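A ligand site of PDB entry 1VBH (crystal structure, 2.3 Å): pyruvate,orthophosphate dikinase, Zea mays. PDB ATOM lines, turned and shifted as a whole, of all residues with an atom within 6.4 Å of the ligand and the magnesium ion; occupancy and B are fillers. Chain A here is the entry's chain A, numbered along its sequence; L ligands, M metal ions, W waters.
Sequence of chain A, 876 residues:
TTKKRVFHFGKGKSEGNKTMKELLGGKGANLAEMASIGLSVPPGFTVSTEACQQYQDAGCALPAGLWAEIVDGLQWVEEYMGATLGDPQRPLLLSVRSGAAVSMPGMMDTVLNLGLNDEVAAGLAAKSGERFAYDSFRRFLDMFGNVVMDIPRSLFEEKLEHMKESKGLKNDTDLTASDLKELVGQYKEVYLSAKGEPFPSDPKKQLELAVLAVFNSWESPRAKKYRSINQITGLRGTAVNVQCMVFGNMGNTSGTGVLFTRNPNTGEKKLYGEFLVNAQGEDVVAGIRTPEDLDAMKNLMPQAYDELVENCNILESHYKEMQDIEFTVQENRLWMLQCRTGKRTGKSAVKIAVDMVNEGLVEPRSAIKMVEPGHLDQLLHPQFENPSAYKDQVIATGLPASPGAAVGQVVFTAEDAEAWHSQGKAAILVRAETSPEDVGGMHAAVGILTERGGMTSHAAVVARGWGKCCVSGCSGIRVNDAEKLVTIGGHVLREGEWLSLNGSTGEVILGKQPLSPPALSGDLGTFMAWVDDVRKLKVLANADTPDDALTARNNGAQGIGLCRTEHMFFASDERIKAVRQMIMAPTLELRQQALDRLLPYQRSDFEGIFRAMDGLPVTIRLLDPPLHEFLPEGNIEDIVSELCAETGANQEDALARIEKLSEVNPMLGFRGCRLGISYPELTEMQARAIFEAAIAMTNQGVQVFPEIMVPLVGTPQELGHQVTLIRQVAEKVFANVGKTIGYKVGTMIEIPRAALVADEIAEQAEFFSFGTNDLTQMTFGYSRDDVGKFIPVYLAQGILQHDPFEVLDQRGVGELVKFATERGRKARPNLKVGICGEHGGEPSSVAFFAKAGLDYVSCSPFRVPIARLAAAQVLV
An oxygen (O1) of the ligand lies close to the backbone carbonyl oxygen (O) of Gly 771 (3.2 Å). Leu 562 touches the ligand. Asp 624 touches the ligand (OD2 to O6, 3.6 Å). Met 748 touches the ligand. Cys 836 touches the ligand. Gly 837 touches the ligand. Hydrophobic or aromatic side chains that line the ligand: Leu 562 and Met 748. Of the 22 residues printed, 12 come within 4 Å of the ligand. The nearest printed residue that does not touch the ligand is Arg 671 (4.3 Å).
O of Glu 750 sits close to N of Leu 775. OE2 of Glu 750 is in hydrogen-bond range of N of Leu 712, 2.6 Å away. The side-chain carboxylate (OD1) of Asp 774 lies within salt-bridge range of the guanidinium group (NH1) of Arg 671 (3.4 Å). The backbone NH of Glu 838 is in hydrogen-bond range of the side-chain amide oxygen of Asn 773 (2.9 Å). The side-chain carboxylate (OE2) of Glu 566 lies within salt-bridge range of the guanidinium group (NH2) of Arg 621 (2.9 Å). The backbone carbonyl oxygen (O) of Phe 770 is in hydrogen-bond range of the backbone NH (N) of Cys 836. The side-chain carboxylate (OD1) of Asp 624 is in salt-bridge range of the guanidinium group (NH2) of Arg 671. The side-chain carboxylate (OE1) of Glu 566 is in hydrogen-bond range of the backbone NH (N) of Asp 624 (3.3 Å).
Water W1 lies within hydrogen-bond range of the side-chain carboxylate of Glu 750 (2.6 Å), the side-chain carboxylate of Asp 624 (2.9 Å) and the guanidinium group of Arg 621 (3.3 Å). Water W3 bridges an oxygen (O5) of the ligand (3.1 Å) and the side-chain carboxylate (OD1) of Asp 774 (3.4 Å). Water W2 lies within hydrogen-bond range of the side-chain carboxylate of Glu 838, the backbone carbonyl oxygen of Cys 836, the side-chain amide nitrogen of Asn 773 and the guanidinium group of Arg 564.
Residues that only touch the magnesium ion: Arg 621 (3.98 Å), Asp 624 (3.9 Å), Arg 671 (3.9 Å) and Met 748 (3.9 Å). Within 4 Å of the magnesium ion: Arg 621, Asp 624, Arg 671, Met 748, Glu 750 and Asp 774. Along chain A the residues within 4 Å of the magnesium ion span positions 621 to 774. The nearest printed residue that does not touch the magnesium ion is Gly 771 (5.4 Å).
O2 of the ligand lies within hydrogen-bond range of N of Asp 774. The guanidinium group (NE) of Arg 564 is in salt-bridge range of an oxygen (O4) of the ligand. The backbone NH (N) of Asn 773 lies within hydrogen-bond range of an oxygen (O1) of the ligand (2.8 Å). ND2 of Asn 773 lies within hydrogen-bond range of O5 of the ligand. The guanidinium group (NH2) of Arg 621 lies within salt-bridge range of an oxygen (O4) of the ligand, at 2.8 Å. N of Thr 772 sits at hydrogen-bond distance from O1 of the ligand (3.2 Å).
The magnesium ion is bound by OE1 of Glu 750 (2.1 Å). OD2 of Asp 774 binds the magnesium ion (2.2 Å). Water W1 binds the magnesium ion, 2.2 Å away. The magnesium ion is bound by O6 of the ligand, at 2.5 Å. Slightly farther from the magnesium ion lies an oxygen (O2) of the ligand (2.7 Å). Slightly farther from the magnesium ion lies O3 of the ligand (2.8 Å).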
ATOM      1  N   ASN A 542     -32.051  17.079   4.671  1.00  0.00           N
ATOM      2  CA  ASN A 542     -31.189  17.123   5.837  1.00  0.00           C
ATOM      3  C   ASN A 542     -30.931  18.614   6.076  1.00  0.00           C
ATOM      4  O   ASN A 542     -30.189  19.261   5.356  1.00  0.00           O
ATOM      5  CB  ASN A 542     -29.845  16.410   5.574  1.00  0.00           C
ATOM      6  CG  ASN A 542     -29.996  14.864   5.490  1.00  0.00           C
ATOM      7  OD1 ASN A 542     -31.023  14.324   5.799  1.00  0.00           O
ATOM      8  ND2 ASN A 542     -28.923  14.194   5.072  1.00  0.00           N
ATOM      9  N   LEU A 562     -33.536  14.589   8.534  1.00  0.00           N
ATOM     10  CA  LEU A 562     -32.502  14.705   9.564  1.00  0.00           C
ATOM     11  C   LEU A 562     -32.126  16.120   9.953  1.00  0.00           C
ATOM     12  O   LEU A 562     -31.554  16.864   9.161  1.00  0.00           O
ATOM     13  CB  LEU A 562     -31.236  13.949   9.151  1.00  0.00           C
ATOM     14  CG  LEU A 562     -30.037  14.026  10.111  1.00  0.00           C
ATOM     15  CD1 LEU A 562     -30.389  13.349  11.419  1.00  0.00           C
ATOM     16  CD2 LEU A 562     -28.822  13.353   9.471  1.00  0.00           C
ATOM     17  N   ARG A 564     -29.827  17.674  12.647  1.00  0.00           N
ATOM     18  CA  ARG A 564     -28.721  17.381  13.578  1.00  0.00           C
ATOM     19  C   ARG A 564     -28.655  18.425  14.710  1.00  0.00           C
ATOM     20  O   ARG A 564     -28.184  19.541  14.498  1.00  0.00           O
ATOM     21  CB  ARG A 564     -27.400  17.388  12.799  1.00  0.00           C
ATOM     22  CG  ARG A 564     -27.155  16.170  11.908  1.00  0.00           C
ATOM     23  CD  ARG A 564     -26.044  16.432  10.886  1.00  0.00           C
ATOM     24  NE  ARG A 564     -25.509  15.199  10.294  1.00  0.00           N
ATOM     25  CZ  ARG A 564     -25.498  14.920   8.984  1.00  0.00           C
ATOM     26  NH1 ARG A 564     -26.013  15.779   8.096  1.00  0.00           N
ATOM     27  NH2 ARG A 564     -24.956  13.784   8.558  1.00  0.00           N
ATOM     28  N   GLU A 566     -26.644  18.813  17.188  1.00  0.00           N
ATOM     29  CA  GLU A 566     -25.326  19.337  17.531  1.00  0.00           C
ATOM     30  C   GLU A 566     -24.973  20.547  16.665  1.00  0.00           C
ATOM     31  O   GLU A 566     -24.361  21.512  17.126  1.00  0.00           O
ATOM     32  CB  GLU A 566     -24.228  18.267  17.402  1.00  0.00           C
ATOM     33  CG  GLU A 566     -24.165  17.508  16.088  1.00  0.00           C
ATOM     34  CD  GLU A 566     -25.150  16.370  16.014  1.00  0.00           C
ATOM     35  OE1 GLU A 566     -26.015  16.273  16.921  1.00  0.00           O
ATOM     36  OE2 GLU A 566     -25.063  15.590  15.053  1.00  0.00           O
ATOM     37  N   HIS A 567     -25.377  20.505  15.402  1.00  0.00           N
ATOM     38  CA  HIS A 567     -25.071  21.601  14.505  1.00  0.00           C
ATOM     39  C   HIS A 567     -25.849  22.875  14.866  1.00  0.00           C
ATOM     40  O   HIS A 567     -25.530  23.952  14.393  1.00  0.00           O
ATOM     41  CB  HIS A 567     -25.339  21.186  13.043  1.00  0.00           C
ATOM     42  CG  HIS A 567     -24.378  20.143  12.520  1.00  0.00           C
ATOM     43  ND1 HIS A 567     -24.504  19.593  11.257  1.00  0.00           N
ATOM     44  CD2 HIS A 567     -23.298  19.574  13.075  1.00  0.00           C
ATOM     45  CE1 HIS A 567     -23.527  18.728  11.066  1.00  0.00           C
ATOM     46  NE2 HIS A 567     -22.769  18.688  12.155  1.00  0.00           N
ATOM     47  N   ARG A 621     -32.853  14.577  15.426  1.00  0.00           N
ATOM     48  CA  ARG A 621     -31.935  13.623  16.051  1.00  0.00           C
ATOM     49  C   ARG A 621     -31.312  14.182  17.336  1.00  0.00           C
ATOM     50  O   ARG A 621     -30.880  15.337  17.375  1.00  0.00           O
ATOM     51  CB  ARG A 621     -30.805  13.251  15.086  1.00  0.00           C
ATOM     52  CG  ARG A 621     -30.038  11.991  15.506  1.00  0.00           C
ATOM     53  CD  ARG A 621     -28.969  11.571  14.487  1.00  0.00           C
ATOM     54  NE  ARG A 621     -27.845  12.510  14.432  1.00  0.00           N
ATOM     55  CZ  ARG A 621     -26.881  12.472  13.483  1.00  0.00           C
ATOM     56  NH1 ARG A 621     -26.921  11.559  12.529  1.00  0.00           N
ATOM     57  NH2 ARG A 621     -25.870  13.327  13.457  1.00  0.00           N
ATOM     58  N   ASP A 624     -25.442  13.897  19.073  1.00  0.00           N
ATOM     59  CA  ASP A 624     -24.609  12.795  18.608  1.00  0.00           C
ATOM     60  C   ASP A 624     -23.057  12.956  18.788  1.00  0.00           C
ATOM     61  O   ASP A 624     -22.387  11.996  19.110  1.00  0.00           O
ATOM     62  CB  ASP A 624     -24.883  12.560  17.103  1.00  0.00           C
ATOM     63  CG  ASP A 624     -23.963  11.477  16.503  1.00  0.00           C
ATOM     64  OD1 ASP A 624     -23.609  10.488  17.217  1.00  0.00           O
ATOM     65  OD2 ASP A 624     -23.583  11.603  15.296  1.00  0.00           O
ATOM     66  N   MET A 667     -14.707   8.649  16.853  1.00  0.00           N
ATOM     67  CA  MET A 667     -15.831   8.197  16.042  1.00  0.00           C
ATOM     68  C   MET A 667     -16.575   7.028  16.708  1.00  0.00           C
ATOM     69  O   MET A 667     -17.757   6.822  16.453  1.00  0.00           O
ATOM     70  CB  MET A 667     -15.361   7.779  14.634  1.00  0.00           C
ATOM     71  CG  MET A 667     -15.244   8.951  13.656  1.00  0.00           C
ATOM     72  SD  MET A 667     -16.847   9.691  13.215  1.00  0.00           S
ATOM     73  CE  MET A 667     -16.521  10.281  11.579  1.00  0.00           C
ATOM     74  N   ARG A 671     -20.256   8.958  22.584  1.00  0.00           N
ATOM     75  CA  ARG A 671     -21.131   9.831  21.817  1.00  0.00           C
ATOM     76  C   ARG A 671     -22.504   9.200  21.561  1.00  0.00           C
ATOM     77  O   ARG A 671     -22.766   8.072  21.978  1.00  0.00           O
ATOM     78  CB  ARG A 671     -20.483  10.238  20.481  1.00  0.00           C
ATOM     79  CG  ARG A 671     -20.086   9.108  19.513  1.00  0.00           C
ATOM     80  CD  ARG A 671     -20.564   9.415  18.068  1.00  0.00           C
ATOM     81  NE  ARG A 671     -19.891   8.641  17.035  1.00  0.00           N
ATOM     82  CZ  ARG A 671     -20.302   8.520  15.774  1.00  0.00           C
ATOM     83  NH1 ARG A 671     -19.600   7.793  14.914  1.00  0.00           N
ATOM     84  NH2 ARG A 671     -21.427   9.099  15.365  1.00  0.00           N
ATOM     85  N   PRO A 711     -29.632   8.500  17.934  1.00  0.00           N
ATOM     86  CA  PRO A 711     -28.371   8.203  17.223  1.00  0.00           C
ATOM     87  C   PRO A 711     -27.545   7.028  17.799  1.00  0.00           C
ATOM     88  O   PRO A 711     -27.573   6.744  19.023  1.00  0.00           O
ATOM     89  CB  PRO A 711     -27.521   9.428  17.418  1.00  0.00           C
ATOM     90  CG  PRO A 711     -28.291  10.377  18.320  1.00  0.00           C
ATOM     91  CD  PRO A 711     -29.604   9.772  18.690  1.00  0.00           C
ATOM     92  N   LEU A 712     -26.793   6.384  16.880  1.00  0.00           N
ATOM     93  CA  LEU A 712     -25.796   5.337  17.203  1.00  0.00           C
ATOM     94  C   LEU A 712     -26.249   4.192  18.117  1.00  0.00           C
ATOM     95  O   LEU A 712     -25.554   3.811  19.060  1.00  0.00           O
ATOM     96  CB  LEU A 712     -24.614   6.041  17.885  1.00  0.00           C
ATOM     97  CG  LEU A 712     -23.245   5.362  17.769  1.00  0.00           C
ATOM     98  CD1 LEU A 712     -22.719   5.388  16.335  1.00  0.00           C
ATOM     99  CD2 LEU A 712     -22.201   6.085  18.632  1.00  0.00           C
ATOM    100  N   MET A 748     -31.649   5.681  14.439  1.00  0.00           N
ATOM    101  CA  MET A 748     -30.677   5.557  13.388  1.00  0.00           C
ATOM    102  C   MET A 748     -30.157   4.117  13.370  1.00  0.00           C
ATOM    103  O   MET A 748     -30.062   3.446  14.387  1.00  0.00           O
ATOM    104  CB  MET A 748     -29.470   6.470  13.679  1.00  0.00           C
ATOM    105  CG  MET A 748     -29.728   7.940  13.368  1.00  0.00           C
ATOM    106  SD  MET A 748     -29.440   8.328  11.665  1.00  0.00           S
ATOM    107  CE  MET A 748     -27.709   8.667  11.710  1.00  0.00           C
ATOM    108  N   GLU A 750     -26.869   2.774  12.123  1.00  0.00           N
ATOM    109  CA  GLU A 750     -25.536   3.076  11.615  1.00  0.00           C
ATOM    110  C   GLU A 750     -24.463   2.186  12.207  1.00  0.00           C
ATOM    111  O   GLU A 750     -23.288   2.272  11.875  1.00  0.00           O
ATOM    112  CB  GLU A 750     -25.166   4.524  11.915  1.00  0.00           C
ATOM    113  CG  GLU A 750     -25.558   4.982  13.306  1.00  0.00           C
ATOM    114  CD  GLU A 750     -25.434   6.515  13.465  1.00  0.00           C
ATOM    115  OE1 GLU A 750     -24.789   7.161  12.600  1.00  0.00           O
ATOM    116  OE2 GLU A 750     -25.980   7.084  14.462  1.00  0.00           O
ATOM    117  N   PHE A 770     -31.180   4.929   8.087  1.00  0.00           N
ATOM    118  CA  PHE A 770     -29.833   4.484   7.847  1.00  0.00           C
ATOM    119  C   PHE A 770     -28.859   5.627   7.727  1.00  0.00           C
ATOM    120  O   PHE A 770     -29.063   6.583   6.958  1.00  0.00           O
ATOM    121  CB  PHE A 770     -29.763   3.668   6.553  1.00  0.00           C
ATOM    122  CG  PHE A 770     -30.392   2.313   6.639  1.00  0.00           C
ATOM    123  CD1 PHE A 770     -29.822   1.299   7.429  1.00  0.00           C
ATOM    124  CD2 PHE A 770     -31.585   2.021   5.941  1.00  0.00           C
ATOM    125  CE1 PHE A 770     -30.414   0.037   7.518  1.00  0.00           C
ATOM    126  CE2 PHE A 770     -32.173   0.760   6.020  1.00  0.00           C
ATOM    127  CZ  PHE A 770     -31.594  -0.232   6.805  1.00  0.00           C
ATOM    128  N   GLY A 771     -27.798   5.497   8.518  1.00  0.00           N
ATOM    129  CA  GLY A 771     -26.692   6.423   8.553  1.00  0.00           C
ATOM    130  C   GLY A 771     -25.533   5.698   7.916  1.00  0.00           C
ATOM    131  O   GLY A 771     -24.600   5.230   8.587  1.00  0.00           O
ATOM    132  N   THR A 772     -25.617   5.609   6.588  1.00  0.00           N
ATOM    133  CA  THR A 772     -24.643   4.933   5.747  1.00  0.00           C
ATOM    134  C   THR A 772     -23.245   5.532   5.847  1.00  0.00           C
ATOM    135  O   THR A 772     -22.259   4.926   5.481  1.00  0.00           O
ATOM    136  CB  THR A 772     -25.093   4.944   4.279  1.00  0.00           C
ATOM    137  OG1 THR A 772     -25.507   6.269   3.940  1.00  0.00           O
ATOM    138  CG2 THR A 772     -26.268   4.016   4.024  1.00  0.00           C
ATOM    139  N   ASN A 773     -23.114   6.751   6.381  1.00  0.00           N
ATOM    140  CA  ASN A 773     -21.780   7.338   6.538  1.00  0.00           C
ATOM    141  C   ASN A 773     -20.992   6.530   7.558  1.00  0.00           C
ATOM    142  O   ASN A 773     -19.886   6.049   7.302  1.00  0.00           O
ATOM    143  CB  ASN A 773     -21.870   8.798   7.057  1.00  0.00           C
ATOM    144  CG  ASN A 773     -22.616   9.732   6.078  1.00  0.00           C
ATOM    145  OD1 ASN A 773     -22.719   9.425   4.912  1.00  0.00           O
ATOM    146  ND2 ASN A 773     -23.092  10.859   6.578  1.00  0.00           N
ATOM    147  N   ASP A 774     -21.629   6.390   8.732  1.00  0.00           N
ATOM    148  CA  ASP A 774     -21.084   5.659   9.854  1.00  0.00           C
ATOM    149  C   ASP A 774     -21.117   4.141   9.617  1.00  0.00           C
ATOM    150  O   ASP A 774     -20.204   3.415   9.982  1.00  0.00           O
ATOM    151  CB  ASP A 774     -21.886   5.981  11.122  1.00  0.00           C
ATOM    152  CG  ASP A 774     -21.365   7.239  11.840  1.00  0.00           C
ATOM    153  OD1 ASP A 774     -20.203   7.676  11.563  1.00  0.00           O
ATOM    154  OD2 ASP A 774     -22.106   7.816  12.704  1.00  0.00           O
ATOM    155  N   LEU A 775     -22.208   3.686   8.986  1.00  0.00           N
ATOM    156  CA  LEU A 775     -22.367   2.273   8.699  1.00  0.00           C
ATOM    157  C   LEU A 775     -21.220   1.799   7.800  1.00  0.00           C
ATOM    158  O   LEU A 775     -20.670   0.702   7.978  1.00  0.00           O
ATOM    159  CB  LEU A 775     -23.700   2.013   7.983  1.00  0.00           C
ATOM    160  CG  LEU A 775     -24.051   0.508   7.909  1.00  0.00           C
ATOM    161  CD1 LEU A 775     -24.109  -0.148   9.288  1.00  0.00           C
ATOM    162  CD2 LEU A 775     -25.419   0.270   7.267  1.00  0.00           C
ATOM    163  N   CYS A 836     -30.331   8.661   5.620  1.00  0.00           N
ATOM    164  CA  CYS A 836     -29.906  10.048   5.686  1.00  0.00           C
ATOM    165  C   CYS A 836     -28.397  10.237   5.505  1.00  0.00           C
ATOM    166  O   CYS A 836     -27.883  11.341   5.622  1.00  0.00           O
ATOM    167  CB  CYS A 836     -30.381  10.713   7.000  1.00  0.00           C
ATOM    168  SG  CYS A 836     -30.045   9.867   8.591  1.00  0.00           S
ATOM    169  N   GLY A 837     -27.687   9.149   5.205  1.00  0.00           N
ATOM    170  CA  GLY A 837     -26.256   9.253   4.960  1.00  0.00           C
ATOM    171  C   GLY A 837     -26.122  10.001   3.634  1.00  0.00           C
ATOM    172  O   GLY A 837     -27.138  10.258   2.996  1.00  0.00           O
ATOM    173  N   GLU A 838     -24.913  10.343   3.206  1.00  0.00           N
ATOM    174  CA  GLU A 838     -24.743  11.095   1.953  1.00  0.00           C
ATOM    175  C   GLU A 838     -25.106  10.346   0.685  1.00  0.00           C
ATOM    176  O   GLU A 838     -25.287  10.931  -0.380  1.00  0.00           O
ATOM    177  CB  GLU A 838     -23.305  11.602   1.853  1.00  0.00           C
ATOM    178  CG  GLU A 838     -22.985  12.572   2.975  1.00  0.00           C
ATOM    179  CD  GLU A 838     -23.787  13.861   2.850  1.00  0.00           C
ATOM    180  OE1 GLU A 838     -23.484  14.640   1.915  1.00  0.00           O
ATOM    181  OE2 GLU A 838     -24.724  14.079   3.671  1.00  0.00           O
HETATM  182  C1  LIG L   1     -24.450   8.964   9.068  1.00  0.00           C
HETATM  183  O1  LIG L   1     -24.709   8.355   7.992  1.00  0.00           O
HETATM  184  O2  LIG L   1     -23.613   8.520   9.741  1.00  0.00           O
HETATM  185  C2  LIG L   1     -25.302  10.254   9.351  1.00  0.00           C
HETATM  186  C3  LIG L   1     -26.280  10.736   8.527  1.00  0.00           C
HETATM  187  O3  LIG L   1     -24.913  10.894  10.567  1.00  0.00           O
HETATM  188  P1  LIG L   1     -23.643  11.911  10.818  1.00  0.00           P
HETATM  189  O4  LIG L   1     -24.084  13.203  11.325  1.00  0.00           O
HETATM  190  O5  LIG L   1     -22.962  12.019   9.517  1.00  0.00           O
HETATM  191  O6  LIG L   1     -22.688  11.176  11.798  1.00  0.00           O
HETATM  192 MG    MG M   1     -23.844   9.050  12.328  1.00  0.00          MG
HETATM  193  O   HOH W   1     -25.045   9.444  14.135  1.00  0.00           O
HETATM  194  O   HOH W   2     -25.348  12.513   5.765  1.00  0.00           O
HETATM  195  O   HOH W   3     -20.347  10.383   9.592  1.00  0.00           O
